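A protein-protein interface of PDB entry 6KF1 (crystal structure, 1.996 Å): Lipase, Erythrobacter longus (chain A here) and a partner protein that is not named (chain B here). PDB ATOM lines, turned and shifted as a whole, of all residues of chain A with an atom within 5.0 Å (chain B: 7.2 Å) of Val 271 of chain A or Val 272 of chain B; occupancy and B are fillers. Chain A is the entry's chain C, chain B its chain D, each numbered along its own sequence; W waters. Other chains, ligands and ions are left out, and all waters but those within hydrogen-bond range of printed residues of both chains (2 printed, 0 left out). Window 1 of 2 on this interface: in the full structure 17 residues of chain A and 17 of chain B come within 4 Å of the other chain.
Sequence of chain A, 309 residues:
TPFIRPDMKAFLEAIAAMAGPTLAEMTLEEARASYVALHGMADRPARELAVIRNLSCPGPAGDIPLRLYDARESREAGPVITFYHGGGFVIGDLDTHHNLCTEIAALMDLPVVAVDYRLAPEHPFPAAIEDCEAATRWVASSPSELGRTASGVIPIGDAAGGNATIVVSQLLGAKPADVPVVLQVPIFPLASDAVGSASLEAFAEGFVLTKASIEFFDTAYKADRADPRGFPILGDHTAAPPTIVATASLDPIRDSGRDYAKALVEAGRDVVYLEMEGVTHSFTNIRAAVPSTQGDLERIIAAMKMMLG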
ATOM      1  N   THR A 243       6.566 -35.991  -3.010  1.00  0.00           N
ATOM      2  CA  THR A 243       6.437 -36.057  -4.471  1.00  0.00           C
ATOM      3  C   THR A 243       7.816 -36.086  -5.110  1.00  0.00           C
ATOM      4  O   THR A 243       8.736 -35.276  -4.715  1.00  0.00           O
ATOM      5  CB  THR A 243       5.593 -34.887  -4.977  1.00  0.00           C
ATOM      6  OG1 THR A 243       4.313 -35.051  -4.368  1.00  0.00           O
ATOM      7  CG2 THR A 243       5.495 -34.919  -6.491  1.00  0.00           C
ATOM      8  N   VAL A 245       8.715 -35.205  -9.028  1.00  0.00           N
ATOM      9  CA  VAL A 245       8.297 -34.765 -10.380  1.00  0.00           C
ATOM     10  C   VAL A 245       9.516 -34.846 -11.287  1.00  0.00           C
ATOM     11  O   VAL A 245      10.525 -34.199 -10.982  1.00  0.00           O
ATOM     12  CB  VAL A 245       7.753 -33.327 -10.431  1.00  0.00           C
ATOM     13  CG1 VAL A 245       7.333 -33.001 -11.872  1.00  0.00           C
ATOM     14  CG2 VAL A 245       6.562 -33.153  -9.493  1.00  0.00           C
ATOM     15  N   ALA A 261       5.329 -28.768  -9.741  1.00  0.00           N
ATOM     16  CA  ALA A 261       6.348 -28.774  -8.668  1.00  0.00           C
ATOM     17  C   ALA A 261       6.376 -27.387  -8.019  1.00  0.00           C
ATOM     18  O   ALA A 261       6.528 -27.296  -6.749  1.00  0.00           O
ATOM     19  CB  ALA A 261       7.737 -29.181  -9.147  1.00  0.00           C
ATOM     20  N   LEU A 264       3.503 -27.275  -5.510  1.00  0.00           N
ATOM     21  CA  LEU A 264       3.834 -28.058  -4.302  1.00  0.00           C
ATOM     22  C   LEU A 264       4.756 -27.221  -3.389  1.00  0.00           C
ATOM     23  O   LEU A 264       4.477 -27.158  -2.186  1.00  0.00           O
ATOM     24  CB  LEU A 264       4.488 -29.382  -4.689  1.00  0.00           C
ATOM     25  CG  LEU A 264       3.574 -30.374  -5.389  1.00  0.00           C
ATOM     26  CD1 LEU A 264       4.265 -31.716  -5.607  1.00  0.00           C
ATOM     27  CD2 LEU A 264       2.295 -30.575  -4.622  1.00  0.00           C
ATOM     28  N   VAL A 265       5.778 -26.565  -3.916  1.00  0.00           N
ATOM     29  CA  VAL A 265       6.678 -25.731  -3.055  1.00  0.00           C
ATOM     30  C   VAL A 265       5.853 -24.579  -2.466  1.00  0.00           C
ATOM     31  O   VAL A 265       5.996 -24.281  -1.260  1.00  0.00           O
ATOM     32  CB  VAL A 265       7.872 -25.196  -3.837  1.00  0.00           C
ATOM     33  CG1 VAL A 265       8.680 -24.204  -3.005  1.00  0.00           C
ATOM     34  CG2 VAL A 265       8.736 -26.295  -4.439  1.00  0.00           C
ATOM     35  N   ARG A 269       5.094 -28.216   0.432  1.00  0.00           N
ATOM     36  CA  ARG A 269       5.137 -29.701   0.411  1.00  0.00           C
ATOM     37  C   ARG A 269       6.537 -30.147  -0.009  1.00  0.00           C
ATOM     38  O   ARG A 269       7.161 -29.444  -0.732  1.00  0.00           O
ATOM     39  CB  ARG A 269       4.078 -30.271  -0.556  1.00  0.00           C
ATOM     40  CG  ARG A 269       2.687 -29.676  -0.362  1.00  0.00           C
ATOM     41  CD  ARG A 269       2.205 -29.730   1.077  1.00  0.00           C
ATOM     42  NE  ARG A 269       2.052 -31.082   1.554  1.00  0.00           N
ATOM     43  CZ  ARG A 269       2.186 -31.470   2.817  1.00  0.00           C
ATOM     44  NH1 ARG A 269       2.483 -30.595   3.765  1.00  0.00           N
ATOM     45  NH2 ARG A 269       2.025 -32.732   3.117  1.00  0.00           N
ATOM     46  N   ASP A 270       6.966 -31.326   0.422  1.00  0.00           N
ATOM     47  CA  ASP A 270       8.280 -31.886   0.055  1.00  0.00           C
ATOM     48  C   ASP A 270       8.217 -32.373  -1.407  1.00  0.00           C
ATOM     49  O   ASP A 270       7.341 -33.192  -1.735  1.00  0.00           O
ATOM     50  CB  ASP A 270       8.655 -32.985   1.028  1.00  0.00           C
ATOM     51  CG  ASP A 270       8.875 -32.504   2.464  1.00  0.00           C
ATOM     52  OD1 ASP A 270       8.983 -31.275   2.708  1.00  0.00           O
ATOM     53  OD2 ASP A 270       8.918 -33.356   3.282  1.00  0.00           O
ATOM     54  N   VAL A 271       9.185 -31.958  -2.217  1.00  0.00           N
ATOM     55  CA  VAL A 271       9.193 -32.336  -3.653  1.00  0.00           C
ATOM     56  C   VAL A 271      10.629 -32.352  -4.131  1.00  0.00           C
ATOM     57  O   VAL A 271      11.403 -31.446  -3.772  1.00  0.00           O
ATOM     58  CB  VAL A 271       8.293 -31.414  -4.492  1.00  0.00           C
ATOM     59  CG1 VAL A 271       8.597 -29.950  -4.303  1.00  0.00           C
ATOM     60  CG2 VAL A 271       8.348 -31.781  -5.977  1.00  0.00           C
ATOM     61  N   VAL A 272      10.954 -33.397  -4.900  1.00  0.00           N
ATOM     62  CA  VAL A 272      12.155 -33.477  -5.759  1.00  0.00           C
ATOM     63  C   VAL A 272      11.724 -33.152  -7.180  1.00  0.00           C
ATOM     64  O   VAL A 272      10.835 -33.859  -7.714  1.00  0.00           O
ATOM     65  CB  VAL A 272      12.762 -34.873  -5.693  1.00  0.00           C
ATOM     66  CG1 VAL A 272      14.009 -34.950  -6.585  1.00  0.00           C
ATOM     67  CG2 VAL A 272      13.046 -35.287  -4.249  1.00  0.00           C
ATOM     68  N   TYR A 273      12.331 -32.137  -7.754  1.00  0.00           N
ATOM     69  CA  TYR A 273      12.086 -31.733  -9.145  1.00  0.00           C
ATOM     70  C   TYR A 273      13.344 -32.092  -9.935  1.00  0.00           C
ATOM     71  O   TYR A 273      14.412 -31.525  -9.665  1.00  0.00           O
ATOM     72  CB  TYR A 273      11.728 -30.265  -9.289  1.00  0.00           C
ATOM     73  CG  TYR A 273      11.464 -29.927 -10.740  1.00  0.00           C
ATOM     74  CD1 TYR A 273      10.338 -30.403 -11.384  1.00  0.00           C
ATOM     75  CD2 TYR A 273      12.416 -29.270 -11.499  1.00  0.00           C
ATOM     76  CE1 TYR A 273      10.099 -30.149 -12.730  1.00  0.00           C
ATOM     77  CE2 TYR A 273      12.224 -29.055 -12.852  1.00  0.00           C
ATOM     78  CZ  TYR A 273      11.073 -29.517 -13.474  1.00  0.00           C
ATOM     79  OH  TYR A 273      10.873 -29.302 -14.793  1.00  0.00           O
ATOM     80  N   MET A 307      13.408 -40.636  -0.861  1.00  0.00           N
ATOM     81  CA  MET A 307      12.140 -40.064  -0.329  1.00  0.00           C
ATOM     82  C   MET A 307      11.358 -41.093   0.489  1.00  0.00           C
ATOM     83  O   MET A 307      10.687 -40.648   1.422  1.00  0.00           O
ATOM     84  CB  MET A 307      11.287 -39.481  -1.444  1.00  0.00           C
ATOM     85  CG  MET A 307      11.928 -38.273  -2.046  1.00  0.00           C
ATOM     86  SD  MET A 307      12.035 -36.868  -0.942  1.00  0.00           S
ATOM     87  CE  MET A 307      10.368 -36.224  -1.110  1.00  0.00           C
ATOM     88  N   PRO B 242      23.320 -24.605 -10.075  1.00  0.00           N
ATOM     89  CA  PRO B 242      23.719 -25.986  -9.840  1.00  0.00           C
ATOM     90  C   PRO B 242      22.614 -26.801  -9.155  1.00  0.00           C
ATOM     91  O   PRO B 242      21.669 -26.230  -8.670  1.00  0.00           O
ATOM     92  CB  PRO B 242      24.888 -25.864  -8.871  1.00  0.00           C
ATOM     93  CG  PRO B 242      24.635 -24.557  -8.142  1.00  0.00           C
ATOM     94  CD  PRO B 242      23.855 -23.666  -9.075  1.00  0.00           C
ATOM     95  N   PRO B 243      22.694 -28.154  -9.126  1.00  0.00           N
ATOM     96  CA  PRO B 243      21.747 -28.979  -8.381  1.00  0.00           C
ATOM     97  C   PRO B 243      21.642 -28.403  -6.958  1.00  0.00           C
ATOM     98  O   PRO B 243      22.685 -28.053  -6.414  1.00  0.00           O
ATOM     99  CB  PRO B 243      22.405 -30.377  -8.348  1.00  0.00           C
ATOM    100  CG  PRO B 243      23.232 -30.398  -9.648  1.00  0.00           C
ATOM    101  CD  PRO B 243      23.745 -28.963  -9.745  1.00  0.00           C
ATOM    102  N   THR B 244      20.423 -28.267  -6.443  1.00  0.00           N
ATOM    103  CA  THR B 244      20.122 -27.561  -5.177  1.00  0.00           C
ATOM    104  C   THR B 244      19.292 -28.426  -4.235  1.00  0.00           C
ATOM    105  O   THR B 244      18.364 -29.150  -4.684  1.00  0.00           O
ATOM    106  CB  THR B 244      19.408 -26.248  -5.494  1.00  0.00           C
ATOM    107  OG1 THR B 244      20.302 -25.572  -6.368  1.00  0.00           O
ATOM    108  CG2 THR B 244      19.077 -25.420  -4.260  1.00  0.00           C
ATOM    109  N   ILE B 245      19.600 -28.368  -2.933  1.00  0.00           N
ATOM    110  CA  ILE B 245      18.664 -28.817  -1.881  1.00  0.00           C
ATOM    111  C   ILE B 245      18.315 -27.576  -1.051  1.00  0.00           C
ATOM    112  O   ILE B 245      19.236 -26.986  -0.474  1.00  0.00           O
ATOM    113  CB  ILE B 245      19.285 -29.894  -1.016  1.00  0.00           C
ATOM    114  CG1 ILE B 245      19.675 -31.139  -1.816  1.00  0.00           C
ATOM    115  CG2 ILE B 245      18.388 -30.219   0.175  1.00  0.00           C
ATOM    116  CD1 ILE B 245      20.645 -31.953  -1.092  1.00  0.00           C
ATOM    117  N   VAL B 246      17.065 -27.135  -1.091  1.00  0.00           N
ATOM    118  CA  VAL B 246      16.553 -26.017  -0.252  1.00  0.00           C
ATOM    119  C   VAL B 246      15.836 -26.648   0.932  1.00  0.00           C
ATOM    120  O   VAL B 246      14.876 -27.432   0.718  1.00  0.00           O
ATOM    121  CB  VAL B 246      15.596 -25.108  -1.016  1.00  0.00           C
ATOM    122  CG1 VAL B 246      15.034 -24.064  -0.081  1.00  0.00           C
ATOM    123  CG2 VAL B 246      16.245 -24.459  -2.231  1.00  0.00           C
ATOM    124  N   TYR B 261      12.714 -19.200  -3.631  1.00  0.00           N
ATOM    125  CA  TYR B 261      13.947 -19.664  -4.301  1.00  0.00           C
ATOM    126  C   TYR B 261      13.720 -21.042  -4.964  1.00  0.00           C
ATOM    127  O   TYR B 261      14.172 -21.164  -6.150  1.00  0.00           O
ATOM    128  CB  TYR B 261      15.168 -19.672  -3.381  1.00  0.00           C
ATOM    129  CG  TYR B 261      16.450 -19.905  -4.133  1.00  0.00           C
ATOM    130  CD1 TYR B 261      16.895 -19.035  -5.106  1.00  0.00           C
ATOM    131  CD2 TYR B 261      17.209 -21.037  -3.894  1.00  0.00           C
ATOM    132  CE1 TYR B 261      18.036 -19.290  -5.845  1.00  0.00           C
ATOM    133  CE2 TYR B 261      18.358 -21.304  -4.627  1.00  0.00           C
ATOM    134  CZ  TYR B 261      18.768 -20.446  -5.615  1.00  0.00           C
ATOM    135  OH  TYR B 261      19.919 -20.725  -6.289  1.00  0.00           O
ATOM    136  N   ALA B 262      13.162 -22.036  -4.267  1.00  0.00           N
ATOM    137  CA  ALA B 262      12.946 -23.380  -4.862  1.00  0.00           C
ATOM    138  C   ALA B 262      11.976 -23.267  -6.052  1.00  0.00           C
ATOM    139  O   ALA B 262      12.289 -23.811  -7.143  1.00  0.00           O
ATOM    140  CB  ALA B 262      12.490 -24.357  -3.833  1.00  0.00           C
ATOM    141  N   LYS B 263      10.973 -22.416  -5.955  1.00  0.00           N
ATOM    142  CA  LYS B 263      10.064 -22.162  -7.107  1.00  0.00           C
ATOM    143  C   LYS B 263      10.806 -21.536  -8.290  1.00  0.00           C
ATOM    144  O   LYS B 263      10.524 -21.912  -9.439  1.00  0.00           O
ATOM    145  CB  LYS B 263       8.869 -21.299  -6.734  1.00  0.00           C
ATOM    146  CG  LYS B 263       7.922 -21.930  -5.739  1.00  0.00           C
ATOM    147  CD  LYS B 263       6.893 -20.942  -5.282  1.00  0.00           C
ATOM    148  CE  LYS B 263       6.006 -20.488  -6.409  1.00  0.00           C
ATOM    149  NZ  LYS B 263       5.185 -19.340  -6.014  1.00  0.00           N
ATOM    150  N   ALA B 264      11.698 -20.577  -8.072  1.00  0.00           N
ATOM    151  CA  ALA B 264      12.455 -19.937  -9.152  1.00  0.00           C
ATOM    152  C   ALA B 264      13.377 -20.956  -9.829  1.00  0.00           C
ATOM    153  O   ALA B 264      13.546 -20.863 -11.044  1.00  0.00           O
ATOM    154  CB  ALA B 264      13.235 -18.730  -8.675  1.00  0.00           C
ATOM    155  N   LEU B 265      13.919 -21.917  -9.097  1.00  0.00           N
ATOM    156  CA  LEU B 265      14.785 -22.941  -9.702  1.00  0.00           C
ATOM    157  C   LEU B 265      13.931 -23.860 -10.604  1.00  0.00           C
ATOM    158  O   LEU B 265      14.364 -24.095 -11.743  1.00  0.00           O
ATOM    159  CB  LEU B 265      15.528 -23.720  -8.623  1.00  0.00           C
ATOM    160  CG  LEU B 265      16.639 -22.950  -7.908  1.00  0.00           C
ATOM    161  CD1 LEU B 265      17.369 -23.844  -6.924  1.00  0.00           C
ATOM    162  CD2 LEU B 265      17.643 -22.371  -8.864  1.00  0.00           C
ATOM    163  N   VAL B 266      12.747 -24.258 -10.161  1.00  0.00           N
ATOM    164  CA  VAL B 266      11.866 -25.137 -10.976  1.00  0.00           C
ATOM    165  C   VAL B 266      11.482 -24.342 -12.209  1.00  0.00           C
ATOM    166  O   VAL B 266      11.535 -24.899 -13.336  1.00  0.00           O
ATOM    167  CB  VAL B 266      10.665 -25.645 -10.187  1.00  0.00           C
ATOM    168  CG1 VAL B 266       9.724 -26.409 -11.103  1.00  0.00           C
ATOM    169  CG2 VAL B 266      11.067 -26.488  -9.000  1.00  0.00           C
ATOM    170  N   GLU B 267      11.157 -23.076 -12.030  1.00  0.00           N
ATOM    171  CA  GLU B 267      10.729 -22.212 -13.148  1.00  0.00           C
ATOM    172  C   GLU B 267      11.846 -22.178 -14.201  1.00  0.00           C
ATOM    173  O   GLU B 267      11.521 -22.120 -15.401  1.00  0.00           O
ATOM    174  CB  GLU B 267      10.411 -20.782 -12.689  1.00  0.00           C
ATOM    175  CG  GLU B 267      10.190 -19.835 -13.859  1.00  0.00           C
ATOM    176  CD  GLU B 267       8.921 -20.099 -14.667  1.00  0.00           C
ATOM    177  OE1 GLU B 267       8.020 -20.732 -14.175  1.00  0.00           O
ATOM    178  OE2 GLU B 267       8.833 -19.626 -15.769  1.00  0.00           O
ATOM    179  N   GLY B 269      14.032 -24.618 -14.794  1.00  0.00           N
ATOM    180  CA  GLY B 269      14.301 -26.003 -15.218  1.00  0.00           C
ATOM    181  C   GLY B 269      15.495 -26.620 -14.512  1.00  0.00           C
ATOM    182  O   GLY B 269      16.086 -27.557 -15.081  1.00  0.00           O
ATOM    183  N   ARG B 270      15.807 -26.171 -13.290  1.00  0.00           N
ATOM    184  CA  ARG B 270      16.984 -26.675 -12.529  1.00  0.00           C
ATOM    185  C   ARG B 270      16.537 -27.782 -11.587  1.00  0.00           C
ATOM    186  O   ARG B 270      15.422 -27.751 -11.059  1.00  0.00           O
ATOM    187  CB  ARG B 270      17.647 -25.525 -11.773  1.00  0.00           C
ATOM    188  CG  ARG B 270      17.857 -24.254 -12.609  1.00  0.00           C
ATOM    189  CD  ARG B 270      18.546 -24.511 -13.950  1.00  0.00           C
ATOM    190  NE  ARG B 270      19.881 -25.103 -13.737  1.00  0.00           N
ATOM    191  CZ  ARG B 270      20.509 -25.878 -14.620  1.00  0.00           C
ATOM    192  NH1 ARG B 270      19.944 -26.213 -15.777  1.00  0.00           N
ATOM    193  NH2 ARG B 270      21.707 -26.336 -14.342  1.00  0.00           N
ATOM    194  N   ASP B 271      17.413 -28.718 -11.327  1.00  0.00           N
ATOM    195  CA  ASP B 271      17.138 -29.805 -10.384  1.00  0.00           C
ATOM    196  C   ASP B 271      17.140 -29.286  -8.934  1.00  0.00           C
ATOM    197  O   ASP B 271      18.120 -28.654  -8.497  1.00  0.00           O
ATOM    198  CB  ASP B 271      18.145 -30.901 -10.589  1.00  0.00           C
ATOM    199  CG  ASP B 271      18.065 -31.608 -11.941  1.00  0.00           C
ATOM    200  OD1 ASP B 271      17.103 -31.424 -12.684  1.00  0.00           O
ATOM    201  OD2 ASP B 271      18.965 -32.380 -12.181  1.00  0.00           O
ATOM    202  N   VAL B 272      16.078 -29.576  -8.182  1.00  0.00           N
ATOM    203  CA  VAL B 272      15.986 -29.071  -6.795  1.00  0.00           C
ATOM    204  C   VAL B 272      15.209 -30.053  -5.932  1.00  0.00           C
ATOM    205  O   VAL B 272      14.196 -30.646  -6.378  1.00  0.00           O
ATOM    206  CB  VAL B 272      15.399 -27.643  -6.751  1.00  0.00           C
ATOM    207  CG1 VAL B 272      14.168 -27.463  -7.581  1.00  0.00           C
ATOM    208  CG2 VAL B 272      15.096 -27.188  -5.323  1.00  0.00           C
ATOM    209  N   VAL B 273      15.726 -30.245  -4.736  1.00  0.00           N
ATOM    210  CA  VAL B 273      15.009 -30.962  -3.683  1.00  0.00           C
ATOM    211  C   VAL B 273      14.516 -29.869  -2.724  1.00  0.00           C
ATOM    212  O   VAL B 273      15.402 -29.056  -2.246  1.00  0.00           O
ATOM    213  CB  VAL B 273      15.946 -31.935  -2.987  1.00  0.00           C
ATOM    214  CG1 VAL B 273      15.218 -32.614  -1.841  1.00  0.00           C
ATOM    215  CG2 VAL B 273      16.543 -32.945  -3.971  1.00  0.00           C
ATOM    216  N   TYR B 274      13.209 -29.805  -2.506  1.00  0.00           N
ATOM    217  CA  TYR B 274      12.583 -28.846  -1.543  1.00  0.00           C
ATOM    218  C   TYR B 274      12.078 -29.631  -0.341  1.00  0.00           C
ATOM    219  O   TYR B 274      11.253 -30.563  -0.441  1.00  0.00           O
ATOM    220  CB  TYR B 274      11.555 -27.937  -2.211  1.00  0.00           C
ATOM    221  CG  TYR B 274      10.974 -26.958  -1.234  1.00  0.00           C
ATOM    222  CD1 TYR B 274      11.726 -25.872  -0.791  1.00  0.00           C
ATOM    223  CD2 TYR B 274       9.768 -27.216  -0.613  1.00  0.00           C
ATOM    224  CE1 TYR B 274      11.208 -24.979   0.143  1.00  0.00           C
ATOM    225  CE2 TYR B 274       9.288 -26.391   0.394  1.00  0.00           C
ATOM    226  CZ  TYR B 274      10.001 -25.253   0.752  1.00  0.00           C
ATOM    227  OH  TYR B 274       9.542 -24.447   1.761  1.00  0.00           O
ATOM    228  N   LEU B 275      12.702 -29.402   0.816  1.00  0.00           N
ATOM    229  CA  LEU B 275      12.262 -30.068   2.071  1.00  0.00           C
ATOM    230  C   LEU B 275      11.816 -28.963   3.049  1.00  0.00           C
ATOM    231  O   LEU B 275      12.668 -28.112   3.431  1.00  0.00           O
ATOM    232  CB  LEU B 275      13.361 -30.927   2.699  1.00  0.00           C
ATOM    233  CG  LEU B 275      13.948 -32.042   1.819  1.00  0.00           C
ATOM    234  CD1 LEU B 275      15.078 -32.731   2.558  1.00  0.00           C
ATOM    235  CD2 LEU B 275      12.909 -33.050   1.408  1.00  0.00           C
ATOM    236  N   GLU B 276      10.575 -29.036   3.518  1.00  0.00           N
ATOM    237  CA  GLU B 276      10.028 -28.041   4.487  1.00  0.00           C
ATOM    238  C   GLU B 276       9.739 -28.814   5.772  1.00  0.00           C
ATOM    239  O   GLU B 276       8.812 -29.657   5.820  1.00  0.00           O
ATOM    240  CB  GLU B 276       8.864 -27.279   3.871  1.00  0.00           C
ATOM    241  CG  GLU B 276       8.216 -26.307   4.847  1.00  0.00           C
ATOM    242  CD  GLU B 276       7.222 -25.348   4.256  1.00  0.00           C
ATOM    243  OE1 GLU B 276       7.518 -24.785   3.189  1.00  0.00           O
ATOM    244  OE2 GLU B 276       6.182 -25.184   4.894  1.00  0.00           O
ATOM    245  N   MET B 308      21.709 -36.577  -4.255  1.00  0.00           N
ATOM    246  CA  MET B 308      21.989 -35.571  -5.311  1.00  0.00           C
ATOM    247  C   MET B 308      23.447 -35.657  -5.804  1.00  0.00           C
ATOM    248  O   MET B 308      23.665 -35.336  -6.963  1.00  0.00           O
ATOM    249  CB  MET B 308      21.610 -34.153  -4.881  1.00  0.00           C
ATOM    250  CG  MET B 308      20.125 -34.019  -4.618  1.00  0.00           C
ATOM    251  SD  MET B 308      19.119 -34.130  -6.167  1.00  0.00           S
ATOM    252  CE  MET B 308      19.543 -32.535  -6.835  1.00  0.00           C
HETATM  253  O   HOH W   1       6.510 -30.349   4.177  1.00  0.00           O
HETATM  254  O   HOH W   2       8.771 -32.389   5.706  1.00  0.00           O
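OD1 of Asp 270 of chain A is in hydrogen-bond range of N of Glu 276 of chain B, 2.9 Å away.
The backbone NH of Tyr 274 of chain B sits at hydrogen-bond distance from the backbone carbonyl oxygen of Val 271 of chain A (2.7 Å).
The backbone NH (N) of Tyr 273 of chain A lies within hydrogen-bond range of the backbone carbonyl oxygen (O) of Val 272 of chain B (2.8 Å).
Hydrophobic or aromatic side chains of chain B that line the printed part of chain A: Ala 262, Val 266 and Tyr 274.
Among the printed residues, 16 pairs touch across the chains.
Among the printed residues, no Asp or Glu carboxylate lies within 4 Å of a Lys or Arg side-chain nitrogen of the other chain.
The backbone carbonyl oxygen (O) of Thr 243 of chain A is in hydrogen-bond range of the backbone NH (N) of Val 272 of chain A, at 2.9 Å.
The backbone NH of Val 245 of chain A is in hydrogen-bond range of the backbone carbonyl oxygen of Val 272 of chain A (2.8 Å).
The backbone carbonyl oxygen of Leu 264 of chain A sits at hydrogen-bond distance from the backbone NH of Arg 269 of chain A (2.9 Å).
N of Thr 244 of chain B is in hydrogen-bond range of O of Asp 271 of chain B, at 3.1 Å.
The backbone NH of Arg 270 of chain B is in hydrogen-bond range of the backbone carbonyl oxygen of Leu 265 of chain B, at 3.0 Å.
The side-chain carboxylate of Glu 276 of chain B is in hydrogen-bond range of the side-chain hydroxyl of Tyr 274 of chain B, at 2.5 Å.
CB of Ala 262 of chain B touches CG1 of Val 265 of chain A, at 3.9 Å.
Val 265 of chain A touches Lys 263 of chain B.
CD2 of Tyr 274 of chain B touches O of Arg 269 of chain A (3.4 Å).
CA of Asp 270 of chain A touches O of Tyr 274 of chain B, 3.3 Å away.
Asp 270 of chain A touches Leu 275 of chain B.
Val 271 of chain A touches Val 272 of chain B.
Val 273 of chain B touches Val 271 of chain A (CA to O, 3.6 Å).
Val 272 of chain B touches Val 272 of chain A (O to CA, 3.5 Å).
Tyr 273 of chain A touches Arg 270 of chain B (CD2 to O, 3.4 Å).
Tyr 273 of chain A touches Asp 271 of chain B.
Printed residues of chain B within 4 Å of Val 265 of chain A: Ala 262 (3.9 Å), Lys 263 (3.6 Å) and Tyr 274 (3.95 Å).
Val 271 of chain A touches three residues of chain B.
Of the printed residues of chain B, Tyr 273 of chain A touches Val 266, Arg 270, Asp 271 and Val 272.
Of the printed residues of chain A, Ala 262 of chain B touches Val 265.
Of chain A, only Val 271, Val 272 and Tyr 273 come within 4 Å of Val 272 of chain B.
Of the printed residues of chain A, Val 273 of chain B touches Val 271.
The nearest residue of chain B that does not touch Val 271 of chain A is Leu 275 of chain B (5.2 Å).
Water W2 lies within hydrogen-bond range of OD2 of Asp 270 of chain A (2.6 Å) and O of Glu 276 of chain B (2.7 Å).
Water W1 lies within hydrogen-bond range of O of Glu 276 of chain B and OD1 of Asp 270 of chain A.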
